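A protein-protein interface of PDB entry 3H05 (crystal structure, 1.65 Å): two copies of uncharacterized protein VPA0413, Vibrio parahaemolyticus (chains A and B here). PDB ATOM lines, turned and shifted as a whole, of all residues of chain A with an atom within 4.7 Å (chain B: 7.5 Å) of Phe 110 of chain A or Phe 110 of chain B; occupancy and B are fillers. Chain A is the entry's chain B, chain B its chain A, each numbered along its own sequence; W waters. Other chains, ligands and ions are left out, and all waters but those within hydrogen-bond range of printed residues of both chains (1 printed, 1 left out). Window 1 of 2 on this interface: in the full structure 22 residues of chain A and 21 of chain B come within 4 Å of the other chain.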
ATOM      1  N   ILE A 105     -25.338  -7.690  -0.228  1.00  0.00           N
ATOM      2  CA  ILE A 105     -25.846  -9.035   0.105  1.00  0.00           C
ATOM      3  C   ILE A 105     -25.698  -9.383   1.587  1.00  0.00           C
ATOM      4  O   ILE A 105     -24.980  -8.702   2.339  1.00  0.00           O
ATOM      5  CB  ILE A 105     -25.136 -10.103  -0.760  1.00  0.00           C
ATOM      6  CG1 ILE A 105     -23.619 -10.089  -0.480  1.00  0.00           C
ATOM      7  CG2 ILE A 105     -25.466  -9.897  -2.233  1.00  0.00           C
ATOM      8  CD1 ILE A 105     -22.797 -11.011  -1.358  1.00  0.00           C
ATOM      9  N   GLY A 106     -26.422 -10.413   2.020  1.00  0.00           N
ATOM     10  CA  GLY A 106     -26.280 -10.980   3.357  1.00  0.00           C
ATOM     11  C   GLY A 106     -25.414 -12.225   3.312  1.00  0.00           C
ATOM     12  O   GLY A 106     -24.947 -12.623   2.233  1.00  0.00           O
ATOM     13  N   PRO A 107     -25.188 -12.852   4.474  1.00  0.00           N
ATOM     14  CA  PRO A 107     -24.216 -13.957   4.561  1.00  0.00           C
ATOM     15  C   PRO A 107     -24.493 -15.164   3.663  1.00  0.00           C
ATOM     16  O   PRO A 107     -23.553 -15.766   3.125  1.00  0.00           O
ATOM     17  CB  PRO A 107     -24.280 -14.377   6.035  1.00  0.00           C
ATOM     18  CG  PRO A 107     -24.883 -13.229   6.744  1.00  0.00           C
ATOM     19  CD  PRO A 107     -25.815 -12.571   5.773  1.00  0.00           C
ATOM     20  N   ASP A 108     -25.760 -15.538   3.522  1.00  0.00           N
ATOM     21  CA  ASP A 108     -26.104 -16.729   2.743  1.00  0.00           C
ATOM     22  C   ASP A 108     -25.794 -16.526   1.264  1.00  0.00           C
ATOM     23  O   ASP A 108     -25.205 -17.399   0.620  1.00  0.00           O
ATOM     24  CB  ASP A 108     -27.559 -17.147   2.965  1.00  0.00           C
ATOM     25  CG  ASP A 108     -28.505 -15.992   2.879  1.00  0.00           C
ATOM     26  OD1 ASP A 108     -28.134 -14.885   3.335  1.00  0.00           O
ATOM     27  OD2 ASP A 108     -29.618 -16.188   2.345  1.00  0.00           O
ATOM     28  N   ASN A 109     -26.154 -15.374   0.711  1.00  0.00           N
ATOM     29  CA  ASN A 109     -25.742 -15.134  -0.654  1.00  0.00           C
ATOM     30  C   ASN A 109     -24.244 -14.893  -0.759  1.00  0.00           C
ATOM     31  O   ASN A 109     -23.643 -15.192  -1.794  1.00  0.00           O
ATOM     32  CB  ASN A 109     -26.536 -13.995  -1.289  1.00  0.00           C
ATOM     33  CG  ASN A 109     -27.931 -14.435  -1.687  1.00  0.00           C
ATOM     34  OD1 ASN A 109     -28.154 -15.588  -2.031  1.00  0.00           O
ATOM     35  ND2 ASN A 109     -28.881 -13.516  -1.615  1.00  0.00           N
ATOM     36  N   PHE A 110     -23.645 -14.352   0.308  1.00  0.00           N
ATOM     37  CA  PHE A 110     -22.211 -14.111   0.323  1.00  0.00           C
ATOM     38  C   PHE A 110     -21.434 -15.383   0.014  1.00  0.00           C
ATOM     39  O   PHE A 110     -20.615 -15.393  -0.904  1.00  0.00           O
ATOM     40  CB  PHE A 110     -21.790 -13.537   1.689  1.00  0.00           C
ATOM     41  CG  PHE A 110     -20.315 -13.254   1.834  1.00  0.00           C
ATOM     42  CD1 PHE A 110     -19.490 -13.009   0.741  1.00  0.00           C
ATOM     43  CD2 PHE A 110     -19.765 -13.194   3.108  1.00  0.00           C
ATOM     44  CE1 PHE A 110     -18.111 -12.757   0.932  1.00  0.00           C
ATOM     45  CE2 PHE A 110     -18.409 -12.895   3.303  1.00  0.00           C
ATOM     46  CZ  PHE A 110     -17.589 -12.675   2.203  1.00  0.00           C
ATOM     47  N   PHE A 111     -21.707 -16.454   0.759  1.00  0.00           N
ATOM     48  CA  PHE A 111     -20.992 -17.712   0.531  1.00  0.00           C
ATOM     49  C   PHE A 111     -21.415 -18.407  -0.781  1.00  0.00           C
ATOM     50  O   PHE A 111     -20.790 -19.387  -1.187  1.00  0.00           O
ATOM     51  CB  PHE A 111     -21.123 -18.666   1.729  1.00  0.00           C
ATOM     52  CG  PHE A 111     -20.347 -18.246   2.965  1.00  0.00           C
ATOM     53  CD1 PHE A 111     -19.549 -17.108   2.973  1.00  0.00           C
ATOM     54  CD2 PHE A 111     -20.364 -19.057   4.105  1.00  0.00           C
ATOM     55  CE1 PHE A 111     -18.820 -16.739   4.127  1.00  0.00           C
ATOM     56  CE2 PHE A 111     -19.641 -18.693   5.255  1.00  0.00           C
ATOM     57  CZ  PHE A 111     -18.885 -17.499   5.250  1.00  0.00           C
ATOM     58  N   LYS A 112     -22.474 -17.911  -1.430  1.00  0.00           N
ATOM     59  CA  LYS A 112     -22.953 -18.471  -2.698  1.00  0.00           C
ATOM     60  C   LYS A 112     -22.722 -17.507  -3.862  1.00  0.00           C
ATOM     61  O   LYS A 112     -23.209 -17.727  -4.961  1.00  0.00           O
ATOM     62  CB  LYS A 112     -24.443 -18.836  -2.601  1.00  0.00           C
ATOM     63  CG  LYS A 112     -24.749 -19.878  -1.536  1.00  0.00           C
ATOM     64  CD  LYS A 112     -26.257 -20.099  -1.357  1.00  0.00           C
ATOM     65  CE  LYS A 112     -26.532 -20.949  -0.119  1.00  0.00           C
ATOM     66  NZ  LYS A 112     -27.996 -21.215   0.083  1.00  0.00           N
ATOM     67  N   PHE A 113     -21.980 -16.427  -3.622  1.00  0.00           N
ATOM     68  CA  PHE A 113     -21.853 -15.374  -4.637  1.00  0.00           C
ATOM     69  C   PHE A 113     -21.191 -15.804  -5.949  1.00  0.00           C
ATOM     70  O   PHE A 113     -21.583 -15.346  -7.014  1.00  0.00           O
ATOM     71  CB  PHE A 113     -21.182 -14.108  -4.055  1.00  0.00           C
ATOM     72  CG  PHE A 113     -21.240 -12.929  -4.983  1.00  0.00           C
ATOM     73  CD1 PHE A 113     -22.457 -12.351  -5.329  1.00  0.00           C
ATOM     74  CD2 PHE A 113     -20.075 -12.402  -5.515  1.00  0.00           C
ATOM     75  CE1 PHE A 113     -22.494 -11.263  -6.215  1.00  0.00           C
ATOM     76  CE2 PHE A 113     -20.115 -11.319  -6.404  1.00  0.00           C
ATOM     77  CZ  PHE A 113     -21.321 -10.758  -6.739  1.00  0.00           C
ATOM     78  N   VAL A 128     -18.974  -4.948  -3.949  1.00  0.00           N
ATOM     79  CA  VAL A 128     -19.938  -5.922  -3.417  1.00  0.00           C
ATOM     80  C   VAL A 128     -19.699  -5.991  -1.900  1.00  0.00           C
ATOM     81  O   VAL A 128     -18.558  -6.149  -1.441  1.00  0.00           O
ATOM     82  CB  VAL A 128     -19.785  -7.327  -4.015  1.00  0.00           C
ATOM     83  CG1 VAL A 128     -20.881  -8.250  -3.462  1.00  0.00           C
ATOM     84  CG2 VAL A 128     -19.928  -7.279  -5.545  1.00  0.00           C
ATOM     85  N   ALA A 130     -20.981  -7.587   1.843  1.00  0.00           N
ATOM     86  CA  ALA A 130     -21.755  -8.568   2.591  1.00  0.00           C
ATOM     87  C   ALA A 130     -21.891  -8.070   4.026  1.00  0.00           C
ATOM     88  O   ALA A 130     -20.906  -8.017   4.772  1.00  0.00           O
ATOM     89  CB  ALA A 130     -21.064  -9.947   2.564  1.00  0.00           C
ATOM     90  N   PHE B 103     -14.360  -4.891   6.707  1.00  0.00           N
ATOM     91  CA  PHE B 103     -13.085  -5.437   6.247  1.00  0.00           C
ATOM     92  C   PHE B 103     -13.060  -5.343   4.726  1.00  0.00           C
ATOM     93  O   PHE B 103     -13.967  -5.848   4.061  1.00  0.00           O
ATOM     94  CB  PHE B 103     -12.968  -6.908   6.683  1.00  0.00           C
ATOM     95  CG  PHE B 103     -11.649  -7.558   6.314  1.00  0.00           C
ATOM     96  CD1 PHE B 103     -10.444  -7.027   6.754  1.00  0.00           C
ATOM     97  CD2 PHE B 103     -11.633  -8.711   5.525  1.00  0.00           C
ATOM     98  CE1 PHE B 103      -9.213  -7.638   6.419  1.00  0.00           C
ATOM     99  CE2 PHE B 103     -10.433  -9.331   5.187  1.00  0.00           C
ATOM    100  CZ  PHE B 103      -9.217  -8.788   5.624  1.00  0.00           C
ATOM    101  N   ILE B 105     -11.514  -6.299   1.188  1.00  0.00           N
ATOM    102  CA  ILE B 105     -10.865  -7.471   0.647  1.00  0.00           C
ATOM    103  C   ILE B 105     -10.763  -7.384  -0.889  1.00  0.00           C
ATOM    104  O   ILE B 105     -11.564  -6.685  -1.516  1.00  0.00           O
ATOM    105  CB  ILE B 105     -11.704  -8.706   1.089  1.00  0.00           C
ATOM    106  CG1 ILE B 105     -10.883  -9.989   1.098  1.00  0.00           C
ATOM    107  CG2 ILE B 105     -12.999  -8.840   0.265  1.00  0.00           C
ATOM    108  CD1 ILE B 105     -11.664 -11.141   1.755  1.00  0.00           C
ATOM    109  N   GLY B 106      -9.843  -8.140  -1.478  1.00  0.00           N
ATOM    110  CA  GLY B 106      -9.796  -8.264  -2.932  1.00  0.00           C
ATOM    111  C   GLY B 106     -10.877  -9.227  -3.390  1.00  0.00           C
ATOM    112  O   GLY B 106     -11.347 -10.059  -2.605  1.00  0.00           O
ATOM    113  N   PRO B 107     -11.300  -9.123  -4.662  1.00  0.00           N
ATOM    114  CA  PRO B 107     -12.343 -10.050  -5.121  1.00  0.00           C
ATOM    115  C   PRO B 107     -11.971 -11.531  -5.041  1.00  0.00           C
ATOM    116  O   PRO B 107     -12.825 -12.346  -4.709  1.00  0.00           O
ATOM    117  CB  PRO B 107     -12.601  -9.594  -6.562  1.00  0.00           C
ATOM    118  CG  PRO B 107     -12.325  -8.107  -6.491  1.00  0.00           C
ATOM    119  CD  PRO B 107     -11.072  -8.042  -5.641  1.00  0.00           C
ATOM    120  N   ASP B 108     -10.713 -11.875  -5.305  1.00  0.00           N
ATOM    121  CA  ASP B 108     -10.268 -13.267  -5.218  1.00  0.00           C
ATOM    122  C   ASP B 108     -10.574 -13.864  -3.850  1.00  0.00           C
ATOM    123  O   ASP B 108     -11.183 -14.940  -3.757  1.00  0.00           O
ATOM    124  CB  ASP B 108      -8.771 -13.400  -5.545  1.00  0.00           C
ATOM    125  CG  ASP B 108      -8.455 -13.179  -7.031  1.00  0.00           C
ATOM    126  OD1 ASP B 108      -9.352 -12.804  -7.821  1.00  0.00           O
ATOM    127  OD2 ASP B 108      -7.282 -13.380  -7.418  1.00  0.00           O
ATOM    128  N   ASN B 109     -10.205 -13.134  -2.791  1.00  0.00           N
ATOM    129  CA  ASN B 109     -10.474 -13.576  -1.430  1.00  0.00           C
ATOM    130  C   ASN B 109     -11.951 -13.504  -1.058  1.00  0.00           C
ATOM    131  O   ASN B 109     -12.427 -14.300  -0.246  1.00  0.00           O
ATOM    132  CB  ASN B 109      -9.617 -12.791  -0.428  1.00  0.00           C
ATOM    133  CG  ASN B 109      -8.175 -13.265  -0.400  1.00  0.00           C
ATOM    134  OD1 ASN B 109      -7.874 -14.411  -0.726  1.00  0.00           O
ATOM    135  ND2 ASN B 109      -7.273 -12.372  -0.020  1.00  0.00           N
ATOM    136  N   PHE B 110     -12.687 -12.554  -1.646  1.00  0.00           N
ATOM    137  CA  PHE B 110     -14.123 -12.478  -1.437  1.00  0.00           C
ATOM    138  C   PHE B 110     -14.780 -13.795  -1.859  1.00  0.00           C
ATOM    139  O   PHE B 110     -15.643 -14.330  -1.153  1.00  0.00           O
ATOM    140  CB  PHE B 110     -14.709 -11.292  -2.232  1.00  0.00           C
ATOM    141  CG  PHE B 110     -16.134 -10.912  -1.852  1.00  0.00           C
ATOM    142  CD1 PHE B 110     -16.375 -10.051  -0.781  1.00  0.00           C
ATOM    143  CD2 PHE B 110     -17.210 -11.417  -2.575  1.00  0.00           C
ATOM    144  CE1 PHE B 110     -17.690  -9.672  -0.441  1.00  0.00           C
ATOM    145  CE2 PHE B 110     -18.533 -11.041  -2.251  1.00  0.00           C
ATOM    146  CZ  PHE B 110     -18.759 -10.161  -1.184  1.00  0.00           C
ATOM    147  N   PHE B 111     -14.357 -14.326  -2.997  1.00  0.00           N
ATOM    148  CA  PHE B 111     -14.953 -15.563  -3.498  1.00  0.00           C
ATOM    149  C   PHE B 111     -14.559 -16.788  -2.685  1.00  0.00           C
ATOM    150  O   PHE B 111     -15.277 -17.786  -2.699  1.00  0.00           O
ATOM    151  CB  PHE B 111     -14.630 -15.764  -4.976  1.00  0.00           C
ATOM    152  CG  PHE B 111     -15.422 -14.868  -5.890  1.00  0.00           C
ATOM    153  CD1 PHE B 111     -16.800 -15.051  -6.053  1.00  0.00           C
ATOM    154  CD2 PHE B 111     -14.799 -13.850  -6.592  1.00  0.00           C
ATOM    155  CE1 PHE B 111     -17.535 -14.220  -6.920  1.00  0.00           C
ATOM    156  CE2 PHE B 111     -15.521 -13.015  -7.451  1.00  0.00           C
ATOM    157  CZ  PHE B 111     -16.895 -13.199  -7.612  1.00  0.00           C
ATOM    158  N   LYS B 112     -13.444 -16.720  -1.963  1.00  0.00           N
ATOM    159  CA  LYS B 112     -13.036 -17.881  -1.158  1.00  0.00           C
ATOM    160  C   LYS B 112     -13.156 -17.631   0.338  1.00  0.00           C
ATOM    161  O   LYS B 112     -12.504 -18.279   1.136  1.00  0.00           O
ATOM    162  CB  LYS B 112     -11.638 -18.350  -1.544  1.00  0.00           C
ATOM    163  CG  LYS B 112     -10.517 -17.340  -1.343  1.00  0.00           C
ATOM    164  CD  LYS B 112      -9.151 -17.929  -1.757  1.00  0.00           C
ATOM    165  CE  LYS B 112      -8.977 -17.935  -3.272  1.00  0.00           C
ATOM    166  NZ  LYS B 112      -7.718 -18.593  -3.730  1.00  0.00           N
ATOM    167  N   PHE B 113     -14.025 -16.702   0.707  1.00  0.00           N
ATOM    168  CA  PHE B 113     -14.108 -16.277   2.104  1.00  0.00           C
ATOM    169  C   PHE B 113     -14.527 -17.399   3.052  1.00  0.00           C
ATOM    170  O   PHE B 113     -14.115 -17.414   4.209  1.00  0.00           O
ATOM    171  CB  PHE B 113     -15.023 -15.045   2.286  1.00  0.00           C
ATOM    172  CG  PHE B 113     -14.738 -14.304   3.552  1.00  0.00           C
ATOM    173  CD1 PHE B 113     -13.618 -13.483   3.626  1.00  0.00           C
ATOM    174  CD2 PHE B 113     -15.534 -14.477   4.687  1.00  0.00           C
ATOM    175  CE1 PHE B 113     -13.299 -12.811   4.784  1.00  0.00           C
ATOM    176  CE2 PHE B 113     -15.203 -13.804   5.887  1.00  0.00           C
ATOM    177  CZ  PHE B 113     -14.090 -12.974   5.921  1.00  0.00           C
ATOM    178  N   ALA B 114     -15.336 -18.338   2.571  1.00  0.00           N
ATOM    179  CA  ALA B 114     -15.818 -19.423   3.428  1.00  0.00           C
ATOM    180  C   ALA B 114     -14.708 -20.267   4.025  1.00  0.00           C
ATOM    181  O   ALA B 114     -14.944 -21.026   4.977  1.00  0.00           O
ATOM    182  CB  ALA B 114     -16.789 -20.310   2.668  1.00  0.00           C
ATOM    183  N   PHE B 116     -11.796 -18.937   5.185  1.00  0.00           N
ATOM    184  CA  PHE B 116     -11.094 -18.112   6.197  1.00  0.00           C
ATOM    185  C   PHE B 116     -11.375 -18.681   7.578  1.00  0.00           C
ATOM    186  O   PHE B 116     -12.483 -19.167   7.854  1.00  0.00           O
ATOM    187  CB  PHE B 116     -11.595 -16.654   6.198  1.00  0.00           C
ATOM    188  CG  PHE B 116     -10.876 -15.703   5.240  1.00  0.00           C
ATOM    189  CD1 PHE B 116     -10.801 -15.971   3.878  1.00  0.00           C
ATOM    190  CD2 PHE B 116     -10.359 -14.486   5.712  1.00  0.00           C
ATOM    191  CE1 PHE B 116     -10.164 -15.080   2.996  1.00  0.00           C
ATOM    192  CE2 PHE B 116      -9.715 -13.567   4.843  1.00  0.00           C
ATOM    193  CZ  PHE B 116      -9.619 -13.875   3.473  1.00  0.00           C
ATOM    194  N   ALA B 119     -14.667 -17.665   9.455  1.00  0.00           N
ATOM    195  CA  ALA B 119     -15.468 -16.949   8.444  1.00  0.00           C
ATOM    196  C   ALA B 119     -16.914 -16.745   8.888  1.00  0.00           C
ATOM    197  O   ALA B 119     -17.435 -15.633   8.770  1.00  0.00           O
ATOM    198  CB  ALA B 119     -15.412 -17.660   7.108  1.00  0.00           C
ATOM    199  N   ILE B 122     -17.143 -14.138  11.555  1.00  0.00           N
ATOM    200  CA  ILE B 122     -16.902 -12.792  10.970  1.00  0.00           C
ATOM    201  C   ILE B 122     -18.182 -12.258  10.359  1.00  0.00           C
ATOM    202  O   ILE B 122     -18.530 -11.078  10.562  1.00  0.00           O
ATOM    203  CB  ILE B 122     -15.743 -12.795   9.948  1.00  0.00           C
ATOM    204  CG1 ILE B 122     -14.422 -13.016  10.683  1.00  0.00           C
ATOM    205  CG2 ILE B 122     -15.674 -11.471   9.112  1.00  0.00           C
ATOM    206  CD1 ILE B 122     -13.250 -13.364   9.759  1.00  0.00           C
ATOM    207  N   THR B 123     -18.905 -13.132   9.645  1.00  0.00           N
ATOM    208  CA  THR B 123     -20.144 -12.714   8.960  1.00  0.00           C
ATOM    209  C   THR B 123     -21.319 -12.504   9.906  1.00  0.00           C
ATOM    210  O   THR B 123     -22.387 -12.040   9.498  1.00  0.00           O
ATOM    211  CB  THR B 123     -20.565 -13.686   7.823  1.00  0.00           C
ATOM    212  OG1 THR B 123     -20.951 -14.943   8.384  1.00  0.00           O
ATOM    213  CG2 THR B 123     -19.440 -13.871   6.795  1.00  0.00           C
ATOM    214  N   TRP B 126     -19.342  -8.489  11.393  1.00  0.00           N
ATOM    215  CA  TRP B 126     -18.687  -7.415  10.619  1.00  0.00           C
ATOM    216  C   TRP B 126     -19.057  -7.474   9.143  1.00  0.00           C
ATOM    217  O   TRP B 126     -19.455  -8.524   8.624  1.00  0.00           O
ATOM    218  CB  TRP B 126     -17.151  -7.477  10.770  1.00  0.00           C
ATOM    219  CG  TRP B 126     -16.742  -7.332  12.208  1.00  0.00           C
ATOM    220  CD1 TRP B 126     -17.005  -6.277  13.018  1.00  0.00           C
ATOM    221  CD2 TRP B 126     -16.082  -8.316  13.018  1.00  0.00           C
ATOM    222  NE1 TRP B 126     -16.522  -6.519  14.283  1.00  0.00           N
ATOM    223  CE2 TRP B 126     -15.948  -7.767  14.309  1.00  0.00           C
ATOM    224  CE3 TRP B 126     -15.577  -9.607  12.766  1.00  0.00           C
ATOM    225  CZ2 TRP B 126     -15.323  -8.447  15.357  1.00  0.00           C
ATOM    226  CZ3 TRP B 126     -14.947 -10.297  13.833  1.00  0.00           C
ATOM    227  CH2 TRP B 126     -14.825  -9.708  15.098  1.00  0.00           C
ATOM    228  N   THR B 127     -18.959  -6.318   8.479  1.00  0.00           N
ATOM    229  CA  THR B 127     -19.192  -6.240   7.036  1.00  0.00           C
ATOM    230  C   THR B 127     -17.911  -6.634   6.318  1.00  0.00           C
ATOM    231  O   THR B 127     -16.814  -6.263   6.751  1.00  0.00           O
ATOM    232  CB  THR B 127     -19.592  -4.800   6.655  1.00  0.00           C
ATOM    233  OG1 THR B 127     -20.844  -4.516   7.307  1.00  0.00           O
ATOM    234  CG2 THR B 127     -19.725  -4.643   5.132  1.00  0.00           C
ATOM    235  N   VAL B 128     -18.063  -7.372   5.219  1.00  0.00           N
ATOM    236  CA  VAL B 128     -16.942  -7.742   4.349  1.00  0.00           C
ATOM    237  C   VAL B 128     -17.232  -7.162   2.964  1.00  0.00           C
ATOM    238  O   VAL B 128     -18.295  -7.387   2.403  1.00  0.00           O
ATOM    239  CB  VAL B 128     -16.730  -9.259   4.293  1.00  0.00           C
ATOM    240  CG1 VAL B 128     -15.540  -9.626   3.341  1.00  0.00           C
ATOM    241  CG2 VAL B 128     -16.538  -9.823   5.714  1.00  0.00           C
ATOM    242  N   MET B 129     -16.285  -6.390   2.443  1.00  0.00           N
ATOM    243  CA  MET B 129     -16.504  -5.566   1.231  1.00  0.00           C
ATOM    244  C   MET B 129     -15.401  -5.811   0.212  1.00  0.00           C
ATOM    245  O   MET B 129     -14.216  -5.665   0.553  1.00  0.00           O
ATOM    246  CB  MET B 129     -16.519  -4.070   1.641  1.00  0.00           C
ATOM    247  CG  MET B 129     -16.486  -3.031   0.495  1.00  0.00           C
ATOM    248  SD  MET B 129     -16.619  -1.253   1.011  1.00  0.00           S
ATOM    249  CE  MET B 129     -18.333  -1.250   1.513  1.00  0.00           C
ATOM    250  N   ALA B 130     -15.764  -6.194  -1.014  1.00  0.00           N
ATOM    251  CA  ALA B 130     -14.810  -6.301  -2.117  1.00  0.00           C
ATOM    252  C   ALA B 130     -14.948  -5.074  -2.976  1.00  0.00           C
ATOM    253  O   ALA B 130     -16.027  -4.805  -3.487  1.00  0.00           O
ATOM    254  CB  ALA B 130     -15.080  -7.524  -2.949  1.00  0.00           C
ATOM    255  N   CYS B 131     -13.869  -4.312  -3.117  1.00  0.00           N
ATOM    256  CA  CYS B 131     -13.908  -3.122  -3.968  1.00  0.00           C
ATOM    257  C   CYS B 131     -13.239  -3.465  -5.290  1.00  0.00           C
ATOM    258  O   CYS B 131     -12.253  -4.206  -5.301  1.00  0.00           O
ATOM    259  CB  CYS B 131     -13.118  -1.979  -3.331  1.00  0.00           C
ATOM    260  SG  CYS B 131     -13.816  -1.423  -1.762  1.00  0.00           S
HETATM  261  O   HOH W   1     -20.269 -10.167   6.524  1.00  0.00           O
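Hydrophobic or aromatic side chains of chain B that line the printed part of chain A: Phe 110, Phe 111, Phe 113, Ala 119 and Val 128.
Among the printed residues, no Asp or Glu carboxylate lies within 4 Å of a Lys or Arg side-chain nitrogen of the other chain.
O of Thr 127 of chain B is in hydrogen-bond range of N of Phe 103 of chain B.
The backbone carbonyl oxygen of Phe 103 of chain B lies within hydrogen-bond range of the backbone NH of Met 129 of chain B (2.9 Å).
The backbone carbonyl oxygen (O) of Met 129 of chain B lies within hydrogen-bond range of the backbone NH (N) of Ile 105 of chain B (2.8 Å).
Pro 107 of chain A touches Thr 123 of chain B.
CE1 of Phe 110 of chain B touches CE1 of Phe 110 of chain A (3.4 Å).
CD2 of Phe 110 of chain A touches CG2 of Thr 123 of chain B, at 3.8 Å.
Phe 110 of chain A touches Val 128 of chain B (CZ to CG1, 3.8 Å).
Phe 111 of chain A touches Ala 119 of chain B (CZ to CB, 3.9 Å).
CE1 of Phe 111 of chain A touches CG2 of Thr 123 of chain B, 3.97 Å away.
Phe 110 of chain B touches Phe 113 of chain A (CE2 to CD2, 3.9 Å).
CG1 of Val 128 of chain A touches CZ of Phe 110 of chain B, at 3.7 Å.
Met 129 of chain B touches Val 128 of chain A.
Thr 127 of chain B touches Ala 130 of chain A.
Phe 110 of chain A touches Phe 113 of chain B, and with the chains exchanged Phe 113 of chain A touches Phe 110 of chain B.
Phe 110 of chain A touches Val 128 of chain B, and with the chains exchanged Val 128 of chain A touches Phe 110 of chain B.
Phe 113 of chain A touches Phe 111 of chain B, but with the chains exchanged Phe 111 of chain A does not touch Phe 113 of chain B (4.03 Å).
Val 128 of chain A touches Ala 130 of chain B, and with the chains exchanged Ala 130 of chain A touches Val 128 of chain B.
Positions printed for both chains: 105, 106, 107, 108, 109, 110, 111, 112, 113, 128 and 130.
Of the 14 pairs that touch across the chains among the printed residues, 7 have their exchanged pair printed and touching as well.
Water W1 lies within hydrogen-bond range of O of Trp 126 of chain B (2.8 Å) and O of Ala 130 of chain A (2.8 Å).
The backbone carbonyl oxygen of Val 128 of chain B is in hydrogen-bond range of the backbone NH of Ala 130 of chain A (2.8 Å).
N of Ala 130 of chain B lies within hydrogen-bond range of O of Val 128 of chain A.
Phe 110 of chain A touches four residues of chain B.
Of the printed residues of chain B, Phe 111 of chain A touches Ala 119 (3.9 Å) and Thr 123 (3.97 Å).
Printed residues of chain B within 4 Å of Phe 113 of chain A: Phe 110 and Phe 111.
Of the printed residues of chain B, Val 128 of chain A touches Phe 110 (3.7 Å), Met 129 (3.4 Å) and Ala 130 (2.8 Å).
Phe 110 of chain B touches just these residues of chain A: Phe 110, Phe 113 and Val 128.
Ile 122 of chain B touches none of the printed residues of chain A.
Of the printed residues of chain A, Met 129 of chain B touches Val 128.
The nearest printed residue of chain B that does not touch Phe 110 of chain A is Phe 111 of chain B (5.7 Å).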
